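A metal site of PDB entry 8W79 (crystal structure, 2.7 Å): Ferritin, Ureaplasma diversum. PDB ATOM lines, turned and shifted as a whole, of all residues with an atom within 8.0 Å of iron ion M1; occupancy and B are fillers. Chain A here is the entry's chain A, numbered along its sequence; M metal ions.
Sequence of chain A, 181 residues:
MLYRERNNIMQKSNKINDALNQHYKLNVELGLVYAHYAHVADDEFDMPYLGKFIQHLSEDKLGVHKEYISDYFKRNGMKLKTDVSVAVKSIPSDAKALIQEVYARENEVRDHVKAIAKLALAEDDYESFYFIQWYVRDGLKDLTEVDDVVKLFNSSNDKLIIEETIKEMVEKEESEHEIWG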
ATOM      1  N   ASN A  27      20.623  -4.870 -12.994  1.00  0.00           N
ATOM      2  CA  ASN A  27      20.266  -5.830 -11.943  1.00  0.00           C
ATOM      3  C   ASN A  27      20.040  -5.143 -10.612  1.00  0.00           C
ATOM      4  O   ASN A  27      19.233  -5.621  -9.808  1.00  0.00           O
ATOM      5  CB  ASN A  27      21.350  -6.892 -11.804  1.00  0.00           C
ATOM      6  CG  ASN A  27      21.209  -7.950 -12.841  1.00  0.00           C
ATOM      7  OD1 ASN A  27      20.375  -8.851 -12.720  1.00  0.00           O
ATOM      8  ND2 ASN A  27      21.960  -7.819 -13.919  1.00  0.00           N
ATOM      9  N   HIS A  56      12.546 -12.999  -3.304  1.00  0.00           N
ATOM     10  CA  HIS A  56      13.708 -13.832  -3.627  1.00  0.00           C
ATOM     11  C   HIS A  56      14.296 -13.444  -4.977  1.00  0.00           C
ATOM     12  O   HIS A  56      15.521 -13.491  -5.161  1.00  0.00           O
ATOM     13  CB  HIS A  56      13.338 -15.320  -3.628  1.00  0.00           C
ATOM     14  CG  HIS A  56      12.995 -15.859  -2.274  1.00  0.00           C
ATOM     15  ND1 HIS A  56      13.412 -15.257  -1.105  1.00  0.00           N
ATOM     16  CD2 HIS A  56      12.280 -16.950  -1.896  1.00  0.00           C
ATOM     17  CE1 HIS A  56      12.969 -15.946  -0.069  1.00  0.00           C
ATOM     18  NE2 HIS A  56      12.281 -16.980  -0.523  1.00  0.00           N
ATOM     19  N   LEU A  57      13.435 -13.075  -5.926  1.00  0.00           N
ATOM     20  CA  LEU A  57      13.945 -12.561  -7.191  1.00  0.00           C
ATOM     21  C   LEU A  57      14.749 -11.286  -6.966  1.00  0.00           C
ATOM     22  O   LEU A  57      15.837 -11.106  -7.528  1.00  0.00           O
ATOM     23  CB  LEU A  57      12.794 -12.326  -8.159  1.00  0.00           C
ATOM     24  CG  LEU A  57      13.003 -12.719  -9.631  1.00  0.00           C
ATOM     25  CD1 LEU A  57      13.514 -14.128  -9.749  1.00  0.00           C
ATOM     26  CD2 LEU A  57      11.695 -12.576 -10.400  1.00  0.00           C
ATOM     27  N   GLU A  59      16.349 -10.297  -4.124  1.00  0.00           N
ATOM     28  CA  GLU A  59      17.623 -10.582  -3.486  1.00  0.00           C
ATOM     29  C   GLU A  59      18.616 -11.246  -4.430  1.00  0.00           C
ATOM     30  O   GLU A  59      19.822 -11.013  -4.323  1.00  0.00           O
ATOM     31  CB  GLU A  59      17.408 -11.452  -2.249  1.00  0.00           C
ATOM     32  CG  GLU A  59      16.812 -10.689  -1.097  1.00  0.00           C
ATOM     33  CD  GLU A  59      16.135 -11.603  -0.085  1.00  0.00           C
ATOM     34  OE1 GLU A  59      15.985 -12.813  -0.377  1.00  0.00           O
ATOM     35  OE2 GLU A  59      15.732 -11.100   0.975  1.00  0.00           O
ATOM     36  N   ASP A  60      18.128 -12.069  -5.362  1.00  0.00           N
ATOM     37  CA  ASP A  60      19.006 -12.639  -6.372  1.00  0.00           C
ATOM     38  C   ASP A  60      19.567 -11.558  -7.288  1.00  0.00           C
ATOM     39  O   ASP A  60      20.765 -11.547  -7.581  1.00  0.00           O
ATOM     40  CB  ASP A  60      18.240 -13.694  -7.165  1.00  0.00           C
ATOM     41  CG  ASP A  60      19.148 -14.579  -7.972  1.00  0.00           C
ATOM     42  OD1 ASP A  60      20.114 -15.133  -7.399  1.00  0.00           O
ATOM     43  OD2 ASP A  60      18.902 -14.724  -9.185  1.00  0.00           O
ATOM     44  N   LYS A  61      18.724 -10.628  -7.742  1.00  0.00           N
ATOM     45  CA  LYS A  61      19.228  -9.622  -8.677  1.00  0.00           C
ATOM     46  C   LYS A  61      20.188  -8.656  -7.991  1.00  0.00           C
ATOM     47  O   LYS A  61      21.220  -8.298  -8.556  1.00  0.00           O
ATOM     48  CB  LYS A  61      18.068  -8.850  -9.349  1.00  0.00           C
ATOM     49  CG  LYS A  61      17.046  -9.754 -10.067  1.00  0.00           C
ATOM     50  CD  LYS A  61      17.240  -9.803 -11.562  1.00  0.00           C
ATOM     51  CE  LYS A  61      16.848 -11.166 -12.141  1.00  0.00           C
ATOM     52  NZ  LYS A  61      17.594 -11.509 -13.398  1.00  0.00           N
ATOM     53  N   VAL A  64      23.937 -12.059  -6.273  1.00  0.00           N
ATOM     54  CA  VAL A  64      24.975 -12.675  -7.082  1.00  0.00           C
ATOM     55  C   VAL A  64      24.975 -12.118  -8.505  1.00  0.00           C
ATOM     56  O   VAL A  64      26.009 -12.177  -9.191  1.00  0.00           O
ATOM     57  CB  VAL A  64      24.808 -14.210  -7.089  1.00  0.00           C
ATOM     58  CG1 VAL A  64      24.886 -14.749  -5.669  1.00  0.00           C
ATOM     59  CG2 VAL A  64      23.501 -14.606  -7.743  1.00  0.00           C
ATOM     60  N   HIS A  65      23.860 -11.571  -8.977  1.00  0.00           N
ATOM     61  CA  HIS A  65      23.838 -11.005 -10.318  1.00  0.00           C
ATOM     62  C   HIS A  65      24.782  -9.805 -10.428  1.00  0.00           C
ATOM     63  O   HIS A  65      25.528  -9.661 -11.407  1.00  0.00           O
ATOM     64  CB  HIS A  65      22.412 -10.620 -10.722  1.00  0.00           C
ATOM     65  CG  HIS A  65      21.579 -11.797 -11.160  1.00  0.00           C
ATOM     66  ND1 HIS A  65      21.253 -12.022 -12.482  1.00  0.00           N
ATOM     67  CD2 HIS A  65      21.010 -12.806 -10.449  1.00  0.00           C
ATOM     68  CE1 HIS A  65      20.507 -13.119 -12.562  1.00  0.00           C
ATOM     69  NE2 HIS A  65      20.351 -13.611 -11.349  1.00  0.00           N
ATOM     70  N   GLU A 106      12.048  -9.804 -17.171  1.00  0.00           N
ATOM     71  CA  GLU A 106      12.962 -10.948 -17.268  1.00  0.00           C
ATOM     72  C   GLU A 106      13.182 -11.370 -18.721  1.00  0.00           C
ATOM     73  O   GLU A 106      14.260 -11.870 -19.053  1.00  0.00           O
ATOM     74  CB  GLU A 106      12.424 -12.116 -16.442  1.00  0.00           C
ATOM     75  CG  GLU A 106      12.446 -11.845 -14.941  1.00  0.00           C
ATOM     76  CD  GLU A 106      13.850 -11.808 -14.402  1.00  0.00           C
ATOM     77  OE1 GLU A 106      14.704 -12.567 -14.878  1.00  0.00           O
ATOM     78  OE2 GLU A 106      14.113 -11.003 -13.487  1.00  0.00           O
ATOM     79  N   VAL A 109      15.853  -9.084 -19.836  1.00  0.00           N
ATOM     80  CA  VAL A 109      17.169  -9.543 -19.390  1.00  0.00           C
ATOM     81  C   VAL A 109      17.781 -10.502 -20.415  1.00  0.00           C
ATOM     82  O   VAL A 109      18.934 -10.335 -20.826  1.00  0.00           O
ATOM     83  CB  VAL A 109      17.093 -10.204 -18.004  1.00  0.00           C
ATOM     84  CG1 VAL A 109      18.398 -10.958 -17.734  1.00  0.00           C
ATOM     85  CG2 VAL A 109      16.811  -9.157 -16.921  1.00  0.00           C
ATOM     86  N   TRP A 134      26.933 -18.208 -17.637  1.00  0.00           N
ATOM     87  CA  TRP A 134      26.062 -18.295 -16.462  1.00  0.00           C
ATOM     88  C   TRP A 134      24.804 -17.456 -16.650  1.00  0.00           C
ATOM     89  O   TRP A 134      23.677 -17.898 -16.374  1.00  0.00           O
ATOM     90  CB  TRP A 134      26.806 -17.834 -15.205  1.00  0.00           C
ATOM     91  CG  TRP A 134      26.059 -18.099 -13.929  1.00  0.00           C
ATOM     92  CD1 TRP A 134      26.081 -19.252 -13.192  1.00  0.00           C
ATOM     93  CD2 TRP A 134      25.170 -17.190 -13.232  1.00  0.00           C
ATOM     94  NE1 TRP A 134      25.273 -19.124 -12.087  1.00  0.00           N
ATOM     95  CE2 TRP A 134      24.700 -17.873 -12.091  1.00  0.00           C
ATOM     96  CE3 TRP A 134      24.734 -15.887 -13.457  1.00  0.00           C
ATOM     97  CZ2 TRP A 134      23.811 -17.290 -11.173  1.00  0.00           C
ATOM     98  CZ3 TRP A 134      23.851 -15.296 -12.542  1.00  0.00           C
ATOM     99  CH2 TRP A 134      23.405 -16.000 -11.416  1.00  0.00           C
ATOM    100  N   TYR A 135      24.966 -16.230 -17.140  1.00  0.00           N
ATOM    101  CA  TYR A 135      23.815 -15.358 -17.340  1.00  0.00           C
ATOM    102  C   TYR A 135      22.906 -15.838 -18.485  1.00  0.00           C
ATOM    103  O   TYR A 135      21.713 -15.540 -18.474  1.00  0.00           O
ATOM    104  CB  TYR A 135      24.306 -13.937 -17.578  1.00  0.00           C
ATOM    105  CG  TYR A 135      24.951 -13.301 -16.363  1.00  0.00           C
ATOM    106  CD1 TYR A 135      26.260 -13.601 -16.011  1.00  0.00           C
ATOM    107  CD2 TYR A 135      24.248 -12.406 -15.578  1.00  0.00           C
ATOM    108  CE1 TYR A 135      26.846 -13.006 -14.881  1.00  0.00           C
ATOM    109  CE2 TYR A 135      24.812 -11.814 -14.478  1.00  0.00           C
ATOM    110  CZ  TYR A 135      26.098 -12.109 -14.125  1.00  0.00           C
ATOM    111  OH  TYR A 135      26.645 -11.500 -13.005  1.00  0.00           O
ATOM    112  N   ARG A 137      21.896 -18.701 -19.024  1.00  0.00           N
ATOM    113  CA  ARG A 137      21.072 -19.744 -18.499  1.00  0.00           C
ATOM    114  C   ARG A 137      20.193 -19.270 -17.370  1.00  0.00           C
ATOM    115  O   ARG A 137      19.069 -19.705 -17.273  1.00  0.00           O
ATOM    116  CB  ARG A 137      22.032 -20.816 -18.024  1.00  0.00           C
ATOM    117  CG  ARG A 137      21.493 -21.833 -17.026  1.00  0.00           C
ATOM    118  CD  ARG A 137      22.483 -22.066 -15.896  1.00  0.00           C
ATOM    119  NE  ARG A 137      22.715 -20.873 -15.080  1.00  0.00           N
ATOM    120  CZ  ARG A 137      21.975 -20.531 -14.033  1.00  0.00           C
ATOM    121  NH1 ARG A 137      20.944 -21.269 -13.656  1.00  0.00           N
ATOM    122  NH2 ARG A 137      22.259 -19.421 -13.369  1.00  0.00           N
ATOM    123  N   ASP A 138      20.680 -18.383 -16.541  1.00  0.00           N
ATOM    124  CA  ASP A 138      19.884 -17.888 -15.438  1.00  0.00           C
ATOM    125  C   ASP A 138      18.767 -17.113 -16.013  1.00  0.00           C
ATOM    126  O   ASP A 138      17.786 -16.912 -15.365  1.00  0.00           O
ATOM    127  CB  ASP A 138      20.698 -16.973 -14.557  1.00  0.00           C
ATOM    128  CG  ASP A 138      20.462 -17.188 -13.088  1.00  0.00           C
ATOM    129  OD1 ASP A 138      19.766 -16.379 -12.446  1.00  0.00           O
ATOM    130  OD2 ASP A 138      21.001 -18.186 -12.575  1.00  0.00           O
ATOM    131  N   GLY A 139      18.933 -16.654 -17.229  1.00  0.00           N
ATOM    132  CA  GLY A 139      17.923 -15.866 -17.853  1.00  0.00           C
ATOM    133  C   GLY A 139      16.795 -16.735 -18.202  1.00  0.00           C
ATOM    134  O   GLY A 139      15.660 -16.385 -17.994  1.00  0.00           O
ATOM    135  N   LYS A 141      16.346 -19.815 -16.791  1.00  0.00           N
ATOM    136  CA  LYS A 141      15.856 -20.395 -15.532  1.00  0.00           C
ATOM    137  C   LYS A 141      14.956 -19.404 -14.786  1.00  0.00           C
ATOM    138  O   LYS A 141      13.832 -19.755 -14.378  1.00  0.00           O
ATOM    139  CB  LYS A 141      17.043 -20.815 -14.658  1.00  0.00           C
ATOM    140  CG  LYS A 141      16.649 -21.479 -13.356  1.00  0.00           C
ATOM    141  CD  LYS A 141      16.927 -20.596 -12.156  1.00  0.00           C
ATOM    142  CE  LYS A 141      18.264 -19.865 -12.259  1.00  0.00           C
ATOM    143  NZ  LYS A 141      18.292 -18.677 -11.342  1.00  0.00           N
ATOM    144  N   ASP A 142      15.423 -18.167 -14.588  1.00  0.00           N
ATOM    145  CA  ASP A 142      14.592 -17.199 -13.887  1.00  0.00           C
ATOM    146  C   ASP A 142      13.311 -16.922 -14.642  1.00  0.00           C
ATOM    147  O   ASP A 142      12.269 -16.671 -14.019  1.00  0.00           O
ATOM    148  CB  ASP A 142      15.346 -15.885 -13.653  1.00  0.00           C
ATOM    149  CG  ASP A 142      16.337 -15.951 -12.500  1.00  0.00           C
ATOM    150  OD1 ASP A 142      16.275 -16.885 -11.669  1.00  0.00           O
ATOM    151  OD2 ASP A 142      17.164 -15.008 -12.396  1.00  0.00           O
ATOM    152  N   LEU A 143      13.357 -16.954 -15.978  1.00  0.00           N
ATOM    153  CA  LEU A 143      12.145 -16.704 -16.741  1.00  0.00           C
ATOM    154  C   LEU A 143      11.142 -17.849 -16.575  1.00  0.00           C
ATOM    155  O   LEU A 143       9.937 -17.612 -16.538  1.00  0.00           O
ATOM    156  CB  LEU A 143      12.482 -16.501 -18.213  1.00  0.00           C
ATOM    157  CG  LEU A 143      11.311 -16.060 -19.113  1.00  0.00           C
ATOM    158  CD1 LEU A 143      11.336 -14.559 -19.262  1.00  0.00           C
ATOM    159  CD2 LEU A 143      11.375 -16.726 -20.481  1.00  0.00           C
ATOM    160  N   GLU A 145      10.824 -19.893 -13.871  1.00  0.00           N
ATOM    161  CA  GLU A 145      10.233 -19.734 -12.546  1.00  0.00           C
ATOM    162  C   GLU A 145       9.094 -18.748 -12.586  1.00  0.00           C
ATOM    163  O   GLU A 145       7.995 -19.022 -12.088  1.00  0.00           O
ATOM    164  CB  GLU A 145      11.275 -19.292 -11.533  1.00  0.00           C
ATOM    165  CG  GLU A 145      12.444 -20.238 -11.325  1.00  0.00           C
ATOM    166  CD  GLU A 145      13.385 -19.718 -10.234  1.00  0.00           C
ATOM    167  OE1 GLU A 145      13.213 -18.551  -9.772  1.00  0.00           O
ATOM    168  OE2 GLU A 145      14.307 -20.480  -9.835  1.00  0.00           O
HETATM  169 FE    FE M   1      18.795 -15.392 -11.218  1.00  0.00          FE
HETATM  170 FE    FE M   2      16.731 -18.556  -7.830  1.00  0.00          FE
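Iron ion M1 is bound by OD1 of Asp 138 (1.9 Å).
Iron ion M1 is bound by OD2 of Asp 142 (2.0 Å).
Iron ion M1 is bound by the side-chain carboxylate (OD2) of Asp 60 (2.1 Å).
NE2 of His 65 binds iron ion M1.
Iron ion M1 has four donor atoms within binding distance.
Merely in contact with iron ion M1: Lys 141 (3.3 Å).
Of the 19 residues printed, 5 come within 4 Å of iron ion M1.
A ring nitrogen (ND1) of His 65 lies within hydrogen-bond range of the side-chain amide oxygen of Asn 27 (3.3 Å).
OD2 of Asp 138 lies within salt-bridge range of NH1 of Arg 137 (3.3 Å).
OD2 of Asp 138 is in salt-bridge range of NZ of Lys 141, at 3.0 Å.
The side-chain carboxylate of Asp 142 lies close to the side-chain amino group of Lys 61 (3.7 Å).
The backbone carbonyl oxygen (O) of His 65 lies within hydrogen-bond range of the side-chain hydroxyl (OH) of Tyr 135 (2.7 Å).
The side-chain amino group (NZ) of Lys 141 lies within salt-bridge range of the side-chain carboxylate (OD1) of Asp 142 (2.7 Å).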
